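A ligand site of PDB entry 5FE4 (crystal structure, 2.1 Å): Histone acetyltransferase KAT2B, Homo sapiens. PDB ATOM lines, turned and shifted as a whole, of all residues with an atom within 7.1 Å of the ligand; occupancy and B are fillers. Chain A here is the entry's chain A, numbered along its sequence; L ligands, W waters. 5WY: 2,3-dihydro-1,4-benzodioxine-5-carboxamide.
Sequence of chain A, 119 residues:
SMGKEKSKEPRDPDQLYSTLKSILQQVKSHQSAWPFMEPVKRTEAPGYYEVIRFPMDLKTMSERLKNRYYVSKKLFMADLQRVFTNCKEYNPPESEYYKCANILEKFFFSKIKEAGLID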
ATOM      1  N   TRP A  34     -12.540 -20.397  14.890  1.00  0.00           N
ATOM      2  CA  TRP A  34     -11.172 -19.944  14.593  1.00  0.00           C
ATOM      3  C   TRP A  34     -10.559 -20.537  13.304  1.00  0.00           C
ATOM      4  O   TRP A  34      -9.875 -19.819  12.617  1.00  0.00           O
ATOM      5  CB  TRP A  34     -10.225 -20.136  15.806  1.00  0.00           C
ATOM      6  CG  TRP A  34      -9.976 -21.571  16.191  1.00  0.00           C
ATOM      7  CD1 TRP A  34     -10.649 -22.294  17.145  1.00  0.00           C
ATOM      8  CD2 TRP A  34      -8.961 -22.452  15.660  1.00  0.00           C
ATOM      9  NE1 TRP A  34     -10.170 -23.571  17.192  1.00  0.00           N
ATOM     10  CE2 TRP A  34      -9.120 -23.688  16.302  1.00  0.00           C
ATOM     11  CE3 TRP A  34      -7.985 -22.316  14.668  1.00  0.00           C
ATOM     12  CZ2 TRP A  34      -8.309 -24.791  16.005  1.00  0.00           C
ATOM     13  CZ3 TRP A  34      -7.142 -23.428  14.372  1.00  0.00           C
ATOM     14  CH2 TRP A  34      -7.314 -24.636  15.050  1.00  0.00           C
ATOM     15  N   PRO A  35     -10.875 -21.801  12.918  1.00  0.00           N
ATOM     16  CA  PRO A  35     -10.292 -22.329  11.683  1.00  0.00           C
ATOM     17  C   PRO A  35     -10.837 -21.706  10.398  1.00  0.00           C
ATOM     18  O   PRO A  35     -10.204 -21.881   9.341  1.00  0.00           O
ATOM     19  CB  PRO A  35     -10.682 -23.809  11.702  1.00  0.00           C
ATOM     20  CG  PRO A  35     -10.912 -24.129  13.102  1.00  0.00           C
ATOM     21  CD  PRO A  35     -11.619 -22.884  13.616  1.00  0.00           C
ATOM     22  N   PHE A  36     -11.961 -20.965  10.505  1.00  0.00           N
ATOM     23  CA  PHE A  36     -12.728 -20.500   9.358  1.00  0.00           C
ATOM     24  C   PHE A  36     -12.758 -19.009   9.217  1.00  0.00           C
ATOM     25  O   PHE A  36     -13.492 -18.479   8.354  1.00  0.00           O
ATOM     26  CB  PHE A  36     -14.178 -21.007   9.499  1.00  0.00           C
ATOM     27  CG  PHE A  36     -14.250 -22.436   9.890  1.00  0.00           C
ATOM     28  CD1 PHE A  36     -13.792 -23.430   9.011  1.00  0.00           C
ATOM     29  CD2 PHE A  36     -14.665 -22.807  11.173  1.00  0.00           C
ATOM     30  CE1 PHE A  36     -13.807 -24.744   9.370  1.00  0.00           C
ATOM     31  CE2 PHE A  36     -14.719 -24.153  11.531  1.00  0.00           C
ATOM     32  CZ  PHE A  36     -14.290 -25.126  10.629  1.00  0.00           C
ATOM     33  N   MET A  37     -11.938 -18.309   9.997  1.00  0.00           N
ATOM     34  CA  MET A  37     -12.036 -16.835  10.092  1.00  0.00           C
ATOM     35  C   MET A  37     -11.538 -16.120   8.802  1.00  0.00           C
ATOM     36  O   MET A  37     -12.037 -15.067   8.449  1.00  0.00           O
ATOM     37  CB  MET A  37     -11.317 -16.306  11.340  1.00  0.00           C
ATOM     38  CG  MET A  37     -12.000 -16.707  12.623  1.00  0.00           C
ATOM     39  SD  MET A  37     -13.645 -15.956  12.876  1.00  0.00           S
ATOM     40  CE  MET A  37     -13.178 -14.220  13.002  1.00  0.00           C
ATOM     41  N   GLU A  38     -10.544 -16.684   8.147  1.00  0.00           N
ATOM     42  CA  GLU A  38      -9.958 -16.069   6.931  1.00  0.00           C
ATOM     43  C   GLU A  38      -9.658 -17.142   5.916  1.00  0.00           C
ATOM     44  O   GLU A  38      -9.638 -18.295   6.283  1.00  0.00           O
ATOM     45  CB  GLU A  38      -8.650 -15.356   7.297  1.00  0.00           C
ATOM     46  CG  GLU A  38      -8.825 -14.374   8.409  1.00  0.00           C
ATOM     47  CD  GLU A  38      -7.719 -13.363   8.521  1.00  0.00           C
ATOM     48  OE1 GLU A  38      -6.520 -13.750   8.420  1.00  0.00           O
ATOM     49  OE2 GLU A  38      -8.080 -12.165   8.698  1.00  0.00           O
ATOM     50  N   PRO A  39      -9.361 -16.778   4.655  1.00  0.00           N
ATOM     51  CA  PRO A  39      -8.902 -17.797   3.701  1.00  0.00           C
ATOM     52  C   PRO A  39      -7.798 -18.686   4.247  1.00  0.00           C
ATOM     53  O   PRO A  39      -6.851 -18.203   4.879  1.00  0.00           O
ATOM     54  CB  PRO A  39      -8.398 -16.968   2.529  1.00  0.00           C
ATOM     55  CG  PRO A  39      -9.288 -15.753   2.563  1.00  0.00           C
ATOM     56  CD  PRO A  39      -9.443 -15.462   4.021  1.00  0.00           C
ATOM     57  N   VAL A  40      -7.878 -19.956   3.962  1.00  0.00           N
ATOM     58  CA  VAL A  40      -6.820 -20.887   4.332  1.00  0.00           C
ATOM     59  C   VAL A  40      -5.540 -20.383   3.614  1.00  0.00           C
ATOM     60  O   VAL A  40      -5.593 -19.998   2.442  1.00  0.00           O
ATOM     61  CB  VAL A  40      -7.161 -22.322   3.935  1.00  0.00           C
ATOM     62  CG1 VAL A  40      -6.017 -23.255   4.239  1.00  0.00           C
ATOM     63  CG2 VAL A  40      -8.418 -22.795   4.667  1.00  0.00           C
ATOM     64  N   LYS A  41      -4.458 -20.272   4.358  1.00  0.00           N
ATOM     65  CA  LYS A  41      -3.155 -19.858   3.817  1.00  0.00           C
ATOM     66  C   LYS A  41      -2.459 -21.035   3.164  1.00  0.00           C
ATOM     67  O   LYS A  41      -2.473 -22.148   3.678  1.00  0.00           O
ATOM     68  CB  LYS A  41      -2.265 -19.314   4.935  1.00  0.00           C
ATOM     69  CG  LYS A  41      -2.764 -18.006   5.539  1.00  0.00           C
ATOM     70  CD  LYS A  41      -1.827 -17.531   6.661  1.00  0.00           C
ATOM     71  CE  LYS A  41      -2.480 -16.412   7.497  1.00  0.00           C
ATOM     72  NZ  LYS A  41      -1.607 -15.919   8.617  1.00  0.00           N
ATOM     73  N   THR A  43       0.646 -21.643   3.187  1.00  0.00           N
ATOM     74  CA  THR A  43       1.616 -22.160   4.151  1.00  0.00           C
ATOM     75  C   THR A  43       0.957 -23.059   5.197  1.00  0.00           C
ATOM     76  O   THR A  43       1.571 -23.963   5.660  1.00  0.00           O
ATOM     77  CB  THR A  43       2.382 -21.027   4.863  1.00  0.00           C
ATOM     78  OG1 THR A  43       1.451 -20.137   5.474  1.00  0.00           O
ATOM     79  CG2 THR A  43       3.248 -20.286   3.898  1.00  0.00           C
ATOM     80  N   GLU A  44      -0.306 -22.808   5.528  1.00  0.00           N
ATOM     81  CA  GLU A  44      -1.096 -23.654   6.447  1.00  0.00           C
ATOM     82  C   GLU A  44      -1.520 -25.010   5.838  1.00  0.00           C
ATOM     83  O   GLU A  44      -1.704 -26.030   6.548  1.00  0.00           O
ATOM     84  CB  GLU A  44      -2.379 -22.887   6.849  1.00  0.00           C
ATOM     85  CG  GLU A  44      -2.075 -21.808   7.832  1.00  0.00           C
ATOM     86  CD  GLU A  44      -3.244 -20.900   8.147  1.00  0.00           C
ATOM     87  OE1 GLU A  44      -4.286 -20.851   7.431  1.00  0.00           O
ATOM     88  OE2 GLU A  44      -3.095 -20.147   9.106  1.00  0.00           O
ATOM     89  N   ALA A  45      -1.698 -25.011   4.516  1.00  0.00           N
ATOM     90  CA  ALA A  45      -2.181 -26.173   3.807  1.00  0.00           C
ATOM     91  C   ALA A  45      -1.673 -26.149   2.337  1.00  0.00           C
ATOM     92  O   ALA A  45      -2.418 -25.797   1.438  1.00  0.00           O
ATOM     93  CB  ALA A  45      -3.683 -26.167   3.861  1.00  0.00           C
ATOM     94  N   TYR A  48      -3.876 -26.875  -0.907  1.00  0.00           N
ATOM     95  CA  TYR A  48      -5.273 -26.731  -0.554  1.00  0.00           C
ATOM     96  C   TYR A  48      -6.083 -26.272  -1.783  1.00  0.00           C
ATOM     97  O   TYR A  48      -7.128 -26.847  -2.111  1.00  0.00           O
ATOM     98  CB  TYR A  48      -5.456 -25.710   0.573  1.00  0.00           C
ATOM     99  CG  TYR A  48      -6.862 -25.543   1.044  1.00  0.00           C
ATOM    100  CD1 TYR A  48      -7.698 -24.591   0.468  1.00  0.00           C
ATOM    101  CD2 TYR A  48      -7.352 -26.294   2.091  1.00  0.00           C
ATOM    102  CE1 TYR A  48      -9.002 -24.420   0.932  1.00  0.00           C
ATOM    103  CE2 TYR A  48      -8.657 -26.132   2.555  1.00  0.00           C
ATOM    104  CZ  TYR A  48      -9.478 -25.189   1.954  1.00  0.00           C
ATOM    105  OH  TYR A  48     -10.768 -25.008   2.435  1.00  0.00           O
ATOM    106  N   VAL A  83     -18.271 -23.546   3.664  1.00  0.00           N
ATOM    107  CA  VAL A  83     -17.188 -23.467   4.633  1.00  0.00           C
ATOM    108  C   VAL A  83     -17.054 -24.853   5.291  1.00  0.00           C
ATOM    109  O   VAL A  83     -15.935 -25.397   5.433  1.00  0.00           O
ATOM    110  CB  VAL A  83     -17.459 -22.397   5.714  1.00  0.00           C
ATOM    111  CG1 VAL A  83     -16.449 -22.451   6.843  1.00  0.00           C
ATOM    112  CG2 VAL A  83     -17.521 -21.013   5.130  1.00  0.00           C
ATOM    113  N   ASN A  86     -16.072 -27.765   2.568  1.00  0.00           N
ATOM    114  CA  ASN A  86     -14.619 -27.660   2.283  1.00  0.00           C
ATOM    115  C   ASN A  86     -13.808 -28.303   3.399  1.00  0.00           C
ATOM    116  O   ASN A  86     -12.967 -29.157   3.147  1.00  0.00           O
ATOM    117  CB  ASN A  86     -14.200 -26.220   2.097  1.00  0.00           C
ATOM    118  CG  ASN A  86     -14.764 -25.640   0.847  1.00  0.00           C
ATOM    119  OD1 ASN A  86     -15.175 -26.377  -0.039  1.00  0.00           O
ATOM    120  ND2 ASN A  86     -14.708 -24.317   0.716  1.00  0.00           N
ATOM    121  N   CYS A  87     -14.143 -27.946   4.631  1.00  0.00           N
ATOM    122  CA  CYS A  87     -13.420 -28.452   5.757  1.00  0.00           C
ATOM    123  C   CYS A  87     -13.476 -29.991   5.806  1.00  0.00           C
ATOM    124  O   CYS A  87     -12.452 -30.650   5.959  1.00  0.00           O
ATOM    125  CB  CYS A  87     -13.929 -27.803   7.019  1.00  0.00           C
ATOM    126  SG  CYS A  87     -13.047 -28.382   8.483  1.00  0.00           S
ATOM    127  N   LYS A  88     -14.664 -30.558   5.601  1.00  0.00           N
ATOM    128  CA  LYS A  88     -14.844 -32.005   5.710  1.00  0.00           C
ATOM    129  C   LYS A  88     -14.327 -32.799   4.522  1.00  0.00           C
ATOM    130  O   LYS A  88     -13.935 -33.904   4.663  1.00  0.00           O
ATOM    131  CB  LYS A  88     -16.296 -32.311   5.995  1.00  0.00           C
ATOM    132  CG  LYS A  88     -16.792 -31.775   7.321  1.00  0.00           C
ATOM    133  CD  LYS A  88     -18.291 -31.876   7.328  1.00  0.00           C
ATOM    134  CE  LYS A  88     -18.841 -31.552   8.639  1.00  0.00           C
ATOM    135  NZ  LYS A  88     -20.326 -31.488   8.577  1.00  0.00           N
ATOM    136  N   TYR A  90     -11.536 -31.754   2.952  1.00  0.00           N
ATOM    137  CA  TYR A  90     -10.063 -31.628   3.005  1.00  0.00           C
ATOM    138  C   TYR A  90      -9.471 -32.422   4.165  1.00  0.00           C
ATOM    139  O   TYR A  90      -8.477 -33.073   3.984  1.00  0.00           O
ATOM    140  CB  TYR A  90      -9.627 -30.143   3.119  1.00  0.00           C
ATOM    141  CG  TYR A  90      -8.149 -29.943   2.945  1.00  0.00           C
ATOM    142  CD1 TYR A  90      -7.561 -30.089   1.695  1.00  0.00           C
ATOM    143  CD2 TYR A  90      -7.334 -29.642   4.042  1.00  0.00           C
ATOM    144  CE1 TYR A  90      -6.186 -29.903   1.518  1.00  0.00           C
ATOM    145  CE2 TYR A  90      -5.956 -29.519   3.903  1.00  0.00           C
ATOM    146  CZ  TYR A  90      -5.395 -29.605   2.642  1.00  0.00           C
ATOM    147  OH  TYR A  90      -4.062 -29.442   2.497  1.00  0.00           O
ATOM    148  N   ASN A  91     -10.108 -32.364   5.332  1.00  0.00           N
ATOM    149  CA  ASN A  91      -9.562 -32.864   6.571  1.00  0.00           C
ATOM    150  C   ASN A  91     -10.067 -34.253   7.021  1.00  0.00           C
ATOM    151  O   ASN A  91     -11.237 -34.609   6.811  1.00  0.00           O
ATOM    152  CB  ASN A  91      -9.840 -31.856   7.691  1.00  0.00           C
ATOM    153  CG  ASN A  91      -9.208 -30.513   7.432  1.00  0.00           C
ATOM    154  OD1 ASN A  91      -7.976 -30.386   7.479  1.00  0.00           O
ATOM    155  ND2 ASN A  91     -10.020 -29.532   7.058  1.00  0.00           N
ATOM    156  N   TYR A  97     -10.035 -29.714  13.039  1.00  0.00           N
ATOM    157  CA  TYR A  97     -10.730 -28.818  12.130  1.00  0.00           C
ATOM    158  C   TYR A  97     -12.129 -29.406  11.796  1.00  0.00           C
ATOM    159  O   TYR A  97     -13.100 -28.673  11.777  1.00  0.00           O
ATOM    160  CB  TYR A  97      -9.983 -28.552  10.823  1.00  0.00           C
ATOM    161  CG  TYR A  97      -8.620 -27.904  10.962  1.00  0.00           C
ATOM    162  CD1 TYR A  97      -8.413 -26.736  11.727  1.00  0.00           C
ATOM    163  CD2 TYR A  97      -7.558 -28.425  10.300  1.00  0.00           C
ATOM    164  CE1 TYR A  97      -7.122 -26.180  11.850  1.00  0.00           C
ATOM    165  CE2 TYR A  97      -6.303 -27.889  10.402  1.00  0.00           C
ATOM    166  CZ  TYR A  97      -6.074 -26.780  11.158  1.00  0.00           C
ATOM    167  OH  TYR A  97      -4.789 -26.328  11.164  1.00  0.00           O
ATOM    168  N   TYR A  98     -12.185 -30.718  11.554  1.00  0.00           N
ATOM    169  CA  TYR A  98     -13.440 -31.394  11.269  1.00  0.00           C
ATOM    170  C   TYR A  98     -14.366 -31.261  12.499  1.00  0.00           C
ATOM    171  O   TYR A  98     -15.506 -30.866  12.325  1.00  0.00           O
ATOM    172  CB  TYR A  98     -13.197 -32.865  10.874  1.00  0.00           C
ATOM    173  CG  TYR A  98     -14.354 -33.574  10.187  1.00  0.00           C
ATOM    174  CD1 TYR A  98     -15.535 -33.861  10.856  1.00  0.00           C
ATOM    175  CD2 TYR A  98     -14.235 -34.025   8.866  1.00  0.00           C
ATOM    176  CE1 TYR A  98     -16.576 -34.580  10.250  1.00  0.00           C
ATOM    177  CE2 TYR A  98     -15.263 -34.733   8.236  1.00  0.00           C
ATOM    178  CZ  TYR A  98     -16.426 -35.020   8.931  1.00  0.00           C
ATOM    179  OH  TYR A  98     -17.515 -35.672   8.352  1.00  0.00           O
HETATM  180  CAE 5WY L   1      -7.111 -26.742   6.949  1.00  0.00           C
HETATM  181  CAC 5WY L   1      -5.709 -26.813   7.086  1.00  0.00           C
HETATM  182  CAD 5WY L   1      -4.991 -25.812   7.784  1.00  0.00           C
HETATM  183  CAK 5WY L   1      -5.704 -24.758   8.311  1.00  0.00           C
HETATM  184  OAH 5WY L   1      -5.036 -23.765   8.940  1.00  0.00           O
HETATM  185  CAF 5WY L   1      -5.788 -22.952   9.809  1.00  0.00           C
HETATM  186  CAG 5WY L   1      -6.997 -22.497   9.055  1.00  0.00           C
HETATM  187  OAI 5WY L   1      -7.809 -23.630   8.668  1.00  0.00           O
HETATM  188  CAM 5WY L   1      -7.131 -24.697   8.160  1.00  0.00           C
HETATM  189  CAL 5WY L   1      -7.888 -25.690   7.473  1.00  0.00           C
HETATM  190  CAJ 5WY L   1      -9.326 -25.709   7.301  1.00  0.00           C
HETATM  191  OAB 5WY L   1      -9.885 -26.685   6.809  1.00  0.00           O
HETATM  192  NAA 5WY L   1     -10.070 -24.745   7.811  1.00  0.00           N
HETATM  193  O   HOH W   1     -11.543 -26.113   4.563  1.00  0.00           O
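The side-chain amide nitrogen (ND2) of Asn 91 sits at hydrogen-bond distance from an oxygen (OAB) of the ligand. NAA of the ligand lies within hydrogen-bond range of O of Pro 35 (3.2 Å). OAH of the ligand lies close to OH of Tyr 97 (3.4 Å).
Water W1 lies within hydrogen-bond range of the side-chain hydroxyl (OH) of Tyr 48 (2.5 Å), an oxygen (OAB) of the ligand (2.8 Å) and the backbone NH (N) of Cys 87 (3.2 Å).
O of Cys 87 sits at hydrogen-bond distance from ND2 of Asn 91 (2.9 Å). The backbone NH (N) of Lys 41 lies within hydrogen-bond range of the side-chain carboxylate (OE1) of Glu 44. The backbone carbonyl oxygen of Tyr 97 sits at hydrogen-bond distance from the side-chain sulfur of Cys 87 (3.3 Å).
OAH of the ligand sits close to OE1 of Glu 44 (3.4 Å). Ala 45 touches the ligand (CB to CAC, 3.9 Å). Cys 87 touches the ligand. Hydrophobic or aromatic side chains that line the ligand: Ala 45 and Tyr 97. Six residues have an atom within 4 Å of the ligand: Pro 35, Glu 44, Ala 45, Cys 87, Asn 91 and Tyr 97.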
